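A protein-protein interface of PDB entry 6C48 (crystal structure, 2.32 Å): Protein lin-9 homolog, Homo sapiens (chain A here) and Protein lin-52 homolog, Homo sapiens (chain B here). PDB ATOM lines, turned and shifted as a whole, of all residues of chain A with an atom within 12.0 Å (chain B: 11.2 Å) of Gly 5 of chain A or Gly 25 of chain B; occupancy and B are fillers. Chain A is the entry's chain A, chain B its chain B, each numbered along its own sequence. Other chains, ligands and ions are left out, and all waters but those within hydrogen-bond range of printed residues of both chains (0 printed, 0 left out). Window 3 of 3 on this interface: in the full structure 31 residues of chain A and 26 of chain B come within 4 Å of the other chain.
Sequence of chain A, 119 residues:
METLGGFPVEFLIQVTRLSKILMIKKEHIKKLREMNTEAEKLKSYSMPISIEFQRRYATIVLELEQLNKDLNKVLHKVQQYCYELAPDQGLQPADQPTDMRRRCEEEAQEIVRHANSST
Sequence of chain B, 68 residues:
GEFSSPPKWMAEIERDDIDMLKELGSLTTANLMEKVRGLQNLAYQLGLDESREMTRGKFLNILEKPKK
Of the 18 printed residues of chain A, 9 touch a printed residue of chain B.
Hydrophobic or aromatic side chains of chain A that line the printed part of chain B: Leu 4, Phe 7, Phe 11, Leu 12 and Val 15.
Hydrophobic or aromatic side chains of chain B that line the printed part of chain A: Met 20, Leu 21, Leu 24, Leu 32, Met 33, Val 36 and Leu 39.
Among the printed residues, 26 pairs touch across the chains.
The backbone carbonyl oxygen of Leu 12 of chain A lies within hydrogen-bond range of the side-chain hydroxyl of Thr 16 of chain A, at 2.8 Å.
OG1 of Thr 28 of chain B is in hydrogen-bond range of N of Asn 31 of chain B (3.1 Å).
Among the printed residues, pairs that only touch across the chains: Phe 7 of chain A with Leu 27 of chain B (3.0 Å), Ser 19 of chain A with Met 20 of chain B (3.2 Å), Phe 7 of chain A with Thr 29 of chain B (3.3 Å), Gly 5 of chain A with Gly 25 of chain B (3.3 Å), Thr 16 of chain A with Leu 21 of chain B (3.3 Å), Thr 16 of chain A with Leu 24 of chain B (3.5 Å), Leu 12 of chain A with Leu 21 of chain B (3.5 Å), Thr 16 of chain A with Asp 17 of chain B (3.6 Å), Val 15 of chain A with Leu 39 of chain B (3.6 Å), Phe 11 of chain A with Leu 32 of chain B (3.6 Å), Phe 7 of chain A with Leu 32 of chain B (3.6 Å), Leu 12 of chain A with Gly 25 of chain B (3.6 Å), Phe 11 of chain A with Met 33 of chain B (3.6 Å), Val 15 of chain A with Leu 24 of chain B (3.6 Å), Leu 12 of chain A with Leu 24 of chain B (3.7 Å), Ser 19 of chain A with Leu 39 of chain B (3.7 Å), Phe 7 of chain A with Gly 25 of chain B (3.7 Å), Phe 7 of chain A with Thr 28 of chain B (3.7 Å), Leu 12 of chain A with Leu 32 of chain B (3.8 Å), Phe 11 of chain A with Val 36 of chain B (3.8 Å), Thr 16 of chain A with Met 20 of chain B (3.8 Å), Leu 4 of chain A with Leu 21 of chain B (3.8 Å), Ile 13 of chain A with Leu 21 of chain B (3.9 Å), Val 15 of chain A with Val 36 of chain B (3.96 Å), Phe 7 of chain A with Leu 24 of chain B (3.96 Å) and Leu 4 of chain A with Gly 25 of chain B (3.99 Å).
Of chain B, only Gly 25 comes within 4 Å of Gly 5 of chain A.
Of the printed residues of chain A, Gly 25 of chain B touches Leu 4 (3.99 Å), Gly 5 (3.3 Å), Phe 7 (3.7 Å) and Leu 12 (3.6 Å).
No residue of chain B comes within 4 Å of Thr 3 of chain A.
Phe 7 of chain A touches just these residues of chain B: Leu 24, Gly 25, Leu 27, Thr 28, Thr 29 and Leu 32.
Of chain A, only Phe 7 (3.96 Å), Leu 12 (3.7 Å), Val 15 (3.6 Å) and Thr 16 (3.5 Å) come within 4 Å of Leu 24 of chain B.
No residue of chain A comes within 4 Å of Ser 26 of chain B.
Of the printed residues of chain A, Met 33 of chain B touches Phe 11.
Of the printed residues of chain A, Val 36 of chain B touches Phe 11 (3.8 Å) and Val 15 (3.96 Å).
Of the printed residues of chain B, Val 15 of chain A touches Leu 24 (3.6 Å), Val 36 (3.96 Å) and Leu 39 (3.6 Å).
Printed residues of chain A within 4 Å of Leu 39 of chain B: Val 15 (3.6 Å) and Ser 19 (3.7 Å).
Glu 10 of chain A touches none of the printed residues of chain B.
Ile 18 of chain B touches none of the printed residues of chain A.
The nearest printed residue of chain A that does not touch Gly 25 of chain B is Gly 6 of chain A (5.1 Å).
The nearest printed residue of chain A that does not touch Met 20 of chain B is Val 15 of chain A (5.3 Å).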
ATOM      1  N   MET A   1      29.539  15.922  -7.382  1.00  0.00           N
ATOM      2  CA  MET A   1      29.349  17.091  -8.236  1.00  0.00           C
ATOM      3  C   MET A   1      27.876  17.376  -8.539  1.00  0.00           C
ATOM      4  O   MET A   1      27.138  16.499  -8.985  1.00  0.00           O
ATOM      5  CB  MET A   1      30.118  16.945  -9.544  1.00  0.00           C
ATOM      6  CG  MET A   1      30.172  18.257 -10.309  1.00  0.00           C
ATOM      7  SD  MET A   1      31.033  18.124 -11.876  1.00  0.00           S
ATOM      8  CE  MET A   1      29.696  17.526 -12.893  1.00  0.00           C
ATOM      9  N   GLU A   2      27.463  18.610  -8.264  1.00  0.00           N
ATOM     10  CA  GLU A   2      26.103  19.039  -8.547  1.00  0.00           C
ATOM     11  C   GLU A   2      25.904  19.248 -10.044  1.00  0.00           C
ATOM     12  O   GLU A   2      26.759  19.822 -10.721  1.00  0.00           O
ATOM     13  CB  GLU A   2      25.797  20.340  -7.806  1.00  0.00           C
ATOM     14  CG  GLU A   2      25.788  20.261  -6.291  1.00  0.00           C
ATOM     15  CD  GLU A   2      24.782  19.264  -5.712  1.00  0.00           C
ATOM     16  OE1 GLU A   2      23.939  18.688  -6.448  1.00  0.00           O
ATOM     17  OE2 GLU A   2      24.841  19.080  -4.483  1.00  0.00           O
ATOM     18  N   THR A   3      24.791  18.752 -10.567  1.00  0.00           N
ATOM     19  CA  THR A   3      24.537  18.750 -11.995  1.00  0.00           C
ATOM     20  C   THR A   3      23.138  19.279 -12.270  1.00  0.00           C
ATOM     21  O   THR A   3      22.295  19.370 -11.378  1.00  0.00           O
ATOM     22  CB  THR A   3      24.690  17.341 -12.610  1.00  0.00           C
ATOM     23  OG1 THR A   3      23.862  16.413 -11.890  1.00  0.00           O
ATOM     24  CG2 THR A   3      26.145  16.887 -12.584  1.00  0.00           C
ATOM     25  N   LEU A   4      22.922  19.689 -13.510  1.00  0.00           N
ATOM     26  CA  LEU A   4      21.602  20.106 -13.956  1.00  0.00           C
ATOM     27  C   LEU A   4      21.557  19.804 -15.438  1.00  0.00           C
ATOM     28  O   LEU A   4      22.375  20.342 -16.190  1.00  0.00           O
ATOM     29  CB  LEU A   4      21.352  21.601 -13.704  1.00  0.00           C
ATOM     30  CG  LEU A   4      19.962  22.176 -13.994  1.00  0.00           C
ATOM     31  CD1 LEU A   4      18.825  21.321 -13.420  1.00  0.00           C
ATOM     32  CD2 LEU A   4      19.831  23.642 -13.576  1.00  0.00           C
ATOM     33  N   GLY A   5      20.609  18.965 -15.851  1.00  0.00           N
ATOM     34  CA  GLY A   5      20.506  18.548 -17.240  1.00  0.00           C
ATOM     35  C   GLY A   5      21.684  17.773 -17.790  1.00  0.00           C
ATOM     36  O   GLY A   5      21.808  17.640 -19.013  1.00  0.00           O
ATOM     37  N   GLY A   6      22.561  17.257 -16.928  1.00  0.00           N
ATOM     38  CA  GLY A   6      23.745  16.555 -17.377  1.00  0.00           C
ATOM     39  C   GLY A   6      25.022  17.375 -17.352  1.00  0.00           C
ATOM     40  O   GLY A   6      26.104  16.805 -17.525  1.00  0.00           O
ATOM     41  N   PHE A   7      24.928  18.712 -17.131  1.00  0.00           N
ATOM     42  CA  PHE A   7      26.065  19.612 -17.056  1.00  0.00           C
ATOM     43  C   PHE A   7      26.403  19.926 -15.606  1.00  0.00           C
ATOM     44  O   PHE A   7      25.514  19.936 -14.752  1.00  0.00           O
ATOM     45  CB  PHE A   7      25.762  20.922 -17.796  1.00  0.00           C
ATOM     46  CG  PHE A   7      25.320  20.718 -19.206  1.00  0.00           C
ATOM     47  CD1 PHE A   7      26.205  20.240 -20.156  1.00  0.00           C
ATOM     48  CD2 PHE A   7      24.018  20.975 -19.574  1.00  0.00           C
ATOM     49  CE1 PHE A   7      25.806  20.039 -21.446  1.00  0.00           C
ATOM     50  CE2 PHE A   7      23.607  20.773 -20.867  1.00  0.00           C
ATOM     51  CZ  PHE A   7      24.504  20.301 -21.809  1.00  0.00           C
ATOM     52  N   PRO A   8      27.664  20.213 -15.288  1.00  0.00           N
ATOM     53  CA  PRO A   8      27.975  20.726 -13.953  1.00  0.00           C
ATOM     54  C   PRO A   8      27.224  22.031 -13.708  1.00  0.00           C
ATOM     55  O   PRO A   8      27.274  22.962 -14.521  1.00  0.00           O
ATOM     56  CB  PRO A   8      29.493  20.946 -14.000  1.00  0.00           C
ATOM     57  CG  PRO A   8      29.957  20.222 -15.210  1.00  0.00           C
ATOM     58  CD  PRO A   8      28.839  20.242 -16.170  1.00  0.00           C
ATOM     59  N   VAL A   9      26.493  22.079 -12.593  1.00  0.00           N
ATOM     60  CA  VAL A   9      25.603  23.210 -12.368  1.00  0.00           C
ATOM     61  C   VAL A   9      26.383  24.508 -12.166  1.00  0.00           C
ATOM     62  O   VAL A   9      25.874  25.593 -12.463  1.00  0.00           O
ATOM     63  CB  VAL A   9      24.661  22.926 -11.185  1.00  0.00           C
ATOM     64  CG1 VAL A   9      25.420  23.005  -9.881  1.00  0.00           C
ATOM     65  CG2 VAL A   9      23.495  23.914 -11.196  1.00  0.00           C
ATOM     66  N   GLU A  10      27.621  24.439 -11.678  1.00  0.00           N
ATOM     67  CA  GLU A  10      28.348  25.686 -11.471  1.00  0.00           C
ATOM     68  C   GLU A  10      28.795  26.294 -12.799  1.00  0.00           C
ATOM     69  O   GLU A  10      28.935  27.519 -12.904  1.00  0.00           O
ATOM     70  CB  GLU A  10      29.539  25.467 -10.536  1.00  0.00           C
ATOM     71  CG  GLU A  10      30.136  26.777 -10.016  1.00  0.00           C
ATOM     72  CD  GLU A  10      29.152  27.530  -9.118  1.00  0.00           C
ATOM     73  OE1 GLU A  10      28.426  26.872  -8.334  1.00  0.00           O
ATOM     74  OE2 GLU A  10      29.085  28.773  -9.214  1.00  0.00           O
ATOM     75  N   PHE A  11      28.965  25.468 -13.829  1.00  0.00           N
ATOM     76  CA  PHE A  11      29.227  25.976 -15.169  1.00  0.00           C
ATOM     77  C   PHE A  11      28.026  26.749 -15.707  1.00  0.00           C
ATOM     78  O   PHE A  11      28.165  27.890 -16.162  1.00  0.00           O
ATOM     79  CB  PHE A  11      29.578  24.813 -16.096  1.00  0.00           C
ATOM     80  CG  PHE A  11      29.855  25.218 -17.512  1.00  0.00           C
ATOM     81  CD1 PHE A  11      30.810  26.175 -17.801  1.00  0.00           C
ATOM     82  CD2 PHE A  11      29.150  24.655 -18.555  1.00  0.00           C
ATOM     83  CE1 PHE A  11      31.072  26.543 -19.102  1.00  0.00           C
ATOM     84  CE2 PHE A  11      29.404  25.023 -19.857  1.00  0.00           C
ATOM     85  CZ  PHE A  11      30.368  25.966 -20.129  1.00  0.00           C
ATOM     86  N   LEU A  12      26.840  26.131 -15.670  1.00  0.00           N
ATOM     87  CA  LEU A  12      25.618  26.784 -16.131  1.00  0.00           C
ATOM     88  C   LEU A  12      25.344  28.076 -15.379  1.00  0.00           C
ATOM     89  O   LEU A  12      24.755  29.005 -15.942  1.00  0.00           O
ATOM     90  CB  LEU A  12      24.420  25.847 -15.970  1.00  0.00           C
ATOM     91  CG  LEU A  12      24.475  24.450 -16.577  1.00  0.00           C
ATOM     92  CD1 LEU A  12      23.214  23.687 -16.218  1.00  0.00           C
ATOM     93  CD2 LEU A  12      24.662  24.543 -18.087  1.00  0.00           C
ATOM     94  N   ILE A  13      25.725  28.136 -14.103  1.00  0.00           N
ATOM     95  CA  ILE A  13      25.544  29.352 -13.319  1.00  0.00           C
ATOM     96  C   ILE A  13      26.400  30.475 -13.896  1.00  0.00           C
ATOM     97  O   ILE A  13      25.923  31.592 -14.125  1.00  0.00           O
ATOM     98  CB  ILE A  13      25.876  29.074 -11.838  1.00  0.00           C
ATOM     99  CG1 ILE A  13      24.793  28.179 -11.221  1.00  0.00           C
ATOM    100  CG2 ILE A  13      26.010  30.364 -11.041  1.00  0.00           C
ATOM    101  CD1 ILE A  13      25.136  27.641  -9.841  1.00  0.00           C
ATOM    102  N   GLN A  14      27.672  30.182 -14.170  1.00  0.00           N
ATOM    103  CA  GLN A  14      28.566  31.192 -14.714  1.00  0.00           C
ATOM    104  C   GLN A  14      28.113  31.638 -16.097  1.00  0.00           C
ATOM    105  O   GLN A  14      28.259  32.812 -16.450  1.00  0.00           O
ATOM    106  CB  GLN A  14      30.002  30.670 -14.749  1.00  0.00           C
ATOM    107  CG  GLN A  14      30.639  30.450 -13.380  1.00  0.00           C
ATOM    108  CD  GLN A  14      30.481  31.647 -12.439  1.00  0.00           C
ATOM    109  OE1 GLN A  14      30.630  32.806 -12.839  1.00  0.00           O
ATOM    110  NE2 GLN A  14      30.193  31.363 -11.179  1.00  0.00           N
ATOM    111  N   VAL A  15      27.577  30.714 -16.901  1.00  0.00           N
ATOM    112  CA  VAL A  15      27.039  31.101 -18.203  1.00  0.00           C
ATOM    113  C   VAL A  15      25.771  31.935 -18.038  1.00  0.00           C
ATOM    114  O   VAL A  15      25.513  32.866 -18.814  1.00  0.00           O
ATOM    115  CB  VAL A  15      26.792  29.864 -19.078  1.00  0.00           C
ATOM    116  CG1 VAL A  15      26.333  30.291 -20.445  1.00  0.00           C
ATOM    117  CG2 VAL A  15      28.057  29.015 -19.188  1.00  0.00           C
ATOM    118  N   THR A  16      24.936  31.588 -17.060  1.00  0.00           N
ATOM    119  CA  THR A  16      23.784  32.430 -16.767  1.00  0.00           C
ATOM    120  C   THR A  16      24.238  33.842 -16.432  1.00  0.00           C
ATOM    121  O   THR A  16      23.679  34.818 -16.937  1.00  0.00           O
ATOM    122  CB  THR A  16      22.965  31.845 -15.612  1.00  0.00           C
ATOM    123  OG1 THR A  16      22.445  30.563 -15.993  1.00  0.00           O
ATOM    124  CG2 THR A  16      21.807  32.788 -15.251  1.00  0.00           C
ATOM    125  N   ARG A  17      25.271  33.965 -15.594  1.00  0.00           N
ATOM    126  CA  ARG A  17      25.735  35.288 -15.199  1.00  0.00           C
ATOM    127  C   ARG A  17      26.382  36.012 -16.368  1.00  0.00           C
ATOM    128  O   ARG A  17      26.174  37.217 -16.544  1.00  0.00           O
ATOM    129  CB  ARG A  17      26.699  35.179 -14.021  1.00  0.00           C
ATOM    130  CG  ARG A  17      25.989  34.733 -12.781  1.00  0.00           C
ATOM    131  CD  ARG A  17      26.844  34.674 -11.540  1.00  0.00           C
ATOM    132  NE  ARG A  17      25.969  34.340 -10.424  1.00  0.00           N
ATOM    133  CZ  ARG A  17      26.347  33.737  -9.306  1.00  0.00           C
ATOM    134  NH1 ARG A  17      27.611  33.395  -9.130  1.00  0.00           N
ATOM    135  NH2 ARG A  17      25.452  33.469  -8.366  1.00  0.00           N
ATOM    136  N   SER A  19      25.631  35.683 -19.607  1.00  0.00           N
ATOM    137  CA  SER A  19      24.572  36.183 -20.477  1.00  0.00           C
ATOM    138  C   SER A  19      23.897  37.421 -19.896  1.00  0.00           C
ATOM    139  O   SER A  19      23.597  38.373 -20.626  1.00  0.00           O
ATOM    140  CB  SER A  19      23.536  35.092 -20.729  1.00  0.00           C
ATOM    141  OG  SER A  19      22.427  35.659 -21.408  1.00  0.00           O
ATOM    142  N   ASP B  17      16.340  34.724 -13.923  1.00  0.00           N
ATOM    143  CA  ASP B  17      17.712  34.197 -13.815  1.00  0.00           C
ATOM    144  C   ASP B  17      17.731  32.675 -13.648  1.00  0.00           C
ATOM    145  O   ASP B  17      18.463  31.974 -14.355  1.00  0.00           O
ATOM    146  CB  ASP B  17      18.440  34.840 -12.624  1.00  0.00           C
ATOM    147  CG  ASP B  17      19.037  36.218 -12.953  1.00  0.00           C
ATOM    148  OD1 ASP B  17      18.526  36.890 -13.879  1.00  0.00           O
ATOM    149  OD2 ASP B  17      19.990  36.637 -12.257  1.00  0.00           O
ATOM    150  N   ILE B  18      16.946  32.147 -12.701  1.00  0.00           N
ATOM    151  CA  ILE B  18      16.741  30.706 -12.601  1.00  0.00           C
ATOM    152  C   ILE B  18      16.139  30.146 -13.880  1.00  0.00           C
ATOM    153  O   ILE B  18      16.469  29.028 -14.289  1.00  0.00           O
ATOM    154  CB  ILE B  18      15.847  30.368 -11.387  1.00  0.00           C
ATOM    155  CG1 ILE B  18      16.537  30.685 -10.066  1.00  0.00           C
ATOM    156  CG2 ILE B  18      15.408  28.932 -11.428  1.00  0.00           C
ATOM    157  CD1 ILE B  18      15.629  30.430  -8.851  1.00  0.00           C
ATOM    158  N   ASP B  19      15.276  30.909 -14.551  1.00  0.00           N
ATOM    159  CA  ASP B  19      14.713  30.433 -15.810  1.00  0.00           C
ATOM    160  C   ASP B  19      15.790  30.307 -16.877  1.00  0.00           C
ATOM    161  O   ASP B  19      15.794  29.344 -17.653  1.00  0.00           O
ATOM    162  CB  ASP B  19      13.595  31.359 -16.266  1.00  0.00           C
ATOM    163  CG  ASP B  19      12.372  31.273 -15.379  1.00  0.00           C
ATOM    164  OD1 ASP B  19      12.029  30.155 -14.914  1.00  0.00           O
ATOM    165  OD2 ASP B  19      11.761  32.330 -15.128  1.00  0.00           O
ATOM    166  N   MET B  20      16.718  31.266 -16.924  1.00  0.00           N
ATOM    167  CA  MET B  20      17.856  31.156 -17.832  1.00  0.00           C
ATOM    168  C   MET B  20      18.728  29.953 -17.483  1.00  0.00           C
ATOM    169  O   MET B  20      19.173  29.220 -18.372  1.00  0.00           O
ATOM    170  CB  MET B  20      18.681  32.441 -17.792  1.00  0.00           C
ATOM    171  CG  MET B  20      19.962  32.336 -18.591  1.00  0.00           C
ATOM    172  SD  MET B  20      19.646  31.885 -20.313  1.00  0.00           S
ATOM    173  CE  MET B  20      20.781  32.964 -21.171  1.00  0.00           C
ATOM    174  N   LEU B  21      19.003  29.756 -16.189  1.00  0.00           N
ATOM    175  CA  LEU B  21      19.750  28.594 -15.728  1.00  0.00           C
ATOM    176  C   LEU B  21      19.101  27.281 -16.177  1.00  0.00           C
ATOM    177  O   LEU B  21      19.789  26.365 -16.651  1.00  0.00           O
ATOM    178  CB  LEU B  21      19.890  28.657 -14.210  1.00  0.00           C
ATOM    179  CG  LEU B  21      20.480  27.434 -13.513  1.00  0.00           C
ATOM    180  CD1 LEU B  21      21.920  27.237 -13.920  1.00  0.00           C
ATOM    181  CD2 LEU B  21      20.381  27.608 -12.006  1.00  0.00           C
ATOM    182  N   LYS B  22      17.777  27.160 -16.013  1.00  0.00           N
ATOM    183  CA  LYS B  22      17.068  25.982 -16.508  1.00  0.00           C
ATOM    184  C   LYS B  22      17.142  25.895 -18.028  1.00  0.00           C
ATOM    185  O   LYS B  22      17.361  24.813 -18.585  1.00  0.00           O
ATOM    186  CB  LYS B  22      15.609  26.003 -16.047  1.00  0.00           C
ATOM    187  CG  LYS B  22      15.436  25.654 -14.583  1.00  0.00           C
ATOM    188  CD  LYS B  22      14.270  26.381 -13.929  1.00  0.00           C
ATOM    189  CE  LYS B  22      12.926  25.863 -14.416  1.00  0.00           C
ATOM    190  NZ  LYS B  22      12.791  24.398 -14.239  1.00  0.00           N
ATOM    191  N   GLU B  23      16.988  27.029 -18.714  1.00  0.00           N
ATOM    192  CA  GLU B  23      17.068  27.032 -20.171  1.00  0.00           C
ATOM    193  C   GLU B  23      18.403  26.459 -20.643  1.00  0.00           C
ATOM    194  O   GLU B  23      18.443  25.606 -21.536  1.00  0.00           O
ATOM    195  CB  GLU B  23      16.909  28.468 -20.678  1.00  0.00           C
ATOM    196  CG  GLU B  23      17.277  28.712 -22.147  1.00  0.00           C
ATOM    197  CD  GLU B  23      16.917  30.129 -22.620  1.00  0.00           C
ATOM    198  OE1 GLU B  23      17.391  30.528 -23.712  1.00  0.00           O
ATOM    199  OE2 GLU B  23      16.189  30.862 -21.893  1.00  0.00           O
ATOM    200  N   LEU B  24      19.503  26.885 -20.014  1.00  0.00           N
ATOM    201  CA  LEU B  24      20.823  26.375 -20.374  1.00  0.00           C
ATOM    202  C   LEU B  24      20.972  24.879 -20.100  1.00  0.00           C
ATOM    203  O   LEU B  24      21.530  24.148 -20.929  1.00  0.00           O
ATOM    204  CB  LEU B  24      21.898  27.165 -19.632  1.00  0.00           C
ATOM    205  CG  LEU B  24      22.011  28.623 -20.071  1.00  0.00           C
ATOM    206  CD1 LEU B  24      23.030  29.380 -19.213  1.00  0.00           C
ATOM    207  CD2 LEU B  24      22.382  28.683 -21.542  1.00  0.00           C
ATOM    208  N   GLY B  25      20.491  24.405 -18.940  1.00  0.00           N
ATOM    209  CA  GLY B  25      20.609  22.995 -18.595  1.00  0.00           C
ATOM    210  C   GLY B  25      19.820  22.061 -19.492  1.00  0.00           C
ATOM    211  O   GLY B  25      20.121  20.864 -19.552  1.00  0.00           O
ATOM    212  N   SER B  26      18.826  22.580 -20.191  1.00  0.00           N
ATOM    213  CA  SER B  26      17.999  21.797 -21.090  1.00  0.00           C
ATOM    214  C   SER B  26      18.572  21.703 -22.498  1.00  0.00           C
ATOM    215  O   SER B  26      17.941  21.093 -23.366  1.00  0.00           O
ATOM    216  CB  SER B  26      16.608  22.421 -21.166  1.00  0.00           C
ATOM    217  OG  SER B  26      16.676  23.622 -21.922  1.00  0.00           O
ATOM    218  N   LEU B  27      19.729  22.308 -22.754  1.00  0.00           N
ATOM    219  CA  LEU B  27      20.352  22.266 -24.068  1.00  0.00           C
ATOM    220  C   LEU B  27      21.219  21.024 -24.222  1.00  0.00           C
ATOM    221  O   LEU B  27      21.756  20.493 -23.249  1.00  0.00           O
ATOM    222  CB  LEU B  27      21.219  23.508 -24.307  1.00  0.00           C
ATOM    223  CG  LEU B  27      20.638  24.925 -24.211  1.00  0.00           C
ATOM    224  CD1 LEU B  27      21.738  25.949 -24.387  1.00  0.00           C
ATOM    225  CD2 LEU B  27      19.586  25.117 -25.278  1.00  0.00           C
ATOM    226  N   THR B  28      21.384  20.591 -25.466  1.00  0.00           N
ATOM    227  CA  THR B  28      22.434  19.635 -25.782  1.00  0.00           C
ATOM    228  C   THR B  28      23.805  20.244 -25.489  1.00  0.00           C
ATOM    229  O   THR B  28      23.963  21.465 -25.363  1.00  0.00           O
ATOM    230  CB  THR B  28      22.363  19.232 -27.255  1.00  0.00           C
ATOM    231  OG1 THR B  28      22.677  20.377 -28.067  1.00  0.00           O
ATOM    232  CG2 THR B  28      20.959  18.695 -27.620  1.00  0.00           C
ATOM    233  N   THR B  29      24.811  19.372 -25.375  1.00  0.00           N
ATOM    234  CA  THR B  29      26.182  19.838 -25.174  1.00  0.00           C
ATOM    235  C   THR B  29      26.647  20.721 -26.331  1.00  0.00           C
ATOM    236  O   THR B  29      27.261  21.774 -26.116  1.00  0.00           O
ATOM    237  CB  THR B  29      27.117  18.651 -24.988  1.00  0.00           C
ATOM    238  OG1 THR B  29      26.774  17.972 -23.776  1.00  0.00           O
ATOM    239  CG2 THR B  29      28.556  19.122 -24.891  1.00  0.00           C
ATOM    240  N   ALA B  30      26.382  20.297 -27.569  1.00  0.00           N
ATOM    241  CA  ALA B  30      26.762  21.117 -28.714  1.00  0.00           C
ATOM    242  C   ALA B  30      26.109  22.493 -28.651  1.00  0.00           C
ATOM    243  O   ALA B  30      26.767  23.499 -28.919  1.00  0.00           O
ATOM    244  CB  ALA B  30      26.411  20.419 -30.029  1.00  0.00           C
ATOM    245  N   ASN B  31      24.826  22.570 -28.276  1.00  0.00           N
ATOM    246  CA  ASN B  31      24.172  23.879 -28.277  1.00  0.00           C
ATOM    247  C   ASN B  31      24.627  24.753 -27.117  1.00  0.00           C
ATOM    248  O   ASN B  31      24.715  25.978 -27.270  1.00  0.00           O
ATOM    249  CB  ASN B  31      22.654  23.743 -28.256  1.00  0.00           C
ATOM    250  CG  ASN B  31      22.105  23.209 -29.552  1.00  0.00           C
ATOM    251  OD1 ASN B  31      22.749  23.324 -30.594  1.00  0.00           O
ATOM    252  ND2 ASN B  31      20.899  22.650 -29.511  1.00  0.00           N
ATOM    253  N   LEU B  32      24.927  24.154 -25.963  1.00  0.00           N
ATOM    254  CA  LEU B  32      25.491  24.919 -24.858  1.00  0.00           C
ATOM    255  C   LEU B  32      26.833  25.513 -25.248  1.00  0.00           C
ATOM    256  O   LEU B  32      27.113  26.684 -24.963  1.00  0.00           O
ATOM    257  CB  LEU B  32      25.651  24.030 -23.631  1.00  0.00           C
ATOM    258  CG  LEU B  32      26.189  24.696 -22.366  1.00  0.00           C
ATOM    259  CD1 LEU B  32      25.228  25.786 -21.895  1.00  0.00           C
ATOM    260  CD2 LEU B  32      26.429  23.634 -21.286  1.00  0.00           C
ATOM    261  N   MET B  33      27.687  24.702 -25.879  1.00  0.00           N
ATOM    262  CA  MET B  33      28.983  25.191 -26.337  1.00  0.00           C
ATOM    263  C   MET B  33      28.843  26.309 -27.371  1.00  0.00           C
ATOM    264  O   MET B  33      29.561  27.310 -27.286  1.00  0.00           O
ATOM    265  CB  MET B  33      29.831  24.032 -26.860  1.00  0.00           C
ATOM    266  CG  MET B  33      30.231  23.055 -25.764  1.00  0.00           C
ATOM    267  SD  MET B  33      30.938  23.850 -24.302  1.00  0.00           S
ATOM    268  CE  MET B  33      29.779  23.334 -23.034  1.00  0.00           C
ATOM    269  N   LYS B  35      26.469  28.417 -27.488  1.00  0.00           N
ATOM    270  CA  LYS B  35      26.021  29.562 -26.712  1.00  0.00           C
ATOM    271  C   LYS B  35      27.194  30.217 -26.004  1.00  0.00           C
ATOM    272  O   LYS B  35      27.370  31.441 -26.075  1.00  0.00           O
ATOM    273  CB  LYS B  35      24.952  29.111 -25.721  1.00  0.00           C
ATOM    274  CG  LYS B  35      24.187  30.229 -25.050  1.00  0.00           C
ATOM    275  CD  LYS B  35      23.119  30.808 -25.968  1.00  0.00           C
ATOM    276  CE  LYS B  35      22.423  32.000 -25.314  1.00  0.00           C
ATOM    277  NZ  LYS B  35      22.824  33.340 -25.894  1.00  0.00           N
ATOM    278  N   VAL B  36      28.015  29.412 -25.318  1.00  0.00           N
ATOM    279  CA  VAL B  36      29.203  29.939 -24.651  1.00  0.00           C
ATOM    280  C   VAL B  36      30.076  30.698 -25.643  1.00  0.00           C
ATOM    281  O   VAL B  36      30.577  31.790 -25.349  1.00  0.00           O
ATOM    282  CB  VAL B  36      29.977  28.811 -23.957  1.00  0.00           C
ATOM    283  CG1 VAL B  36      31.225  29.370 -23.300  1.00  0.00           C
ATOM    284  CG2 VAL B  36      29.093  28.173 -22.911  1.00  0.00           C
ATOM    285  N   LEU B  39      28.409  33.912 -26.585  1.00  0.00           N
ATOM    286  CA  LEU B  39      28.482  34.877 -25.500  1.00  0.00           C
ATOM    287  C   LEU B  39      29.884  35.442 -25.377  1.00  0.00           C
ATOM    288  O   LEU B  39      30.056  36.626 -25.061  1.00  0.00           O
ATOM    289  CB  LEU B  39      28.048  34.243 -24.183  1.00  0.00           C
ATOM    290  CG  LEU B  39      26.571  33.875 -24.037  1.00  0.00           C
ATOM    291  CD1 LEU B  39      26.405  32.928 -22.858  1.00  0.00           C
ATOM    292  CD2 LEU B  39      25.719  35.110 -23.854  1.00  0.00           C
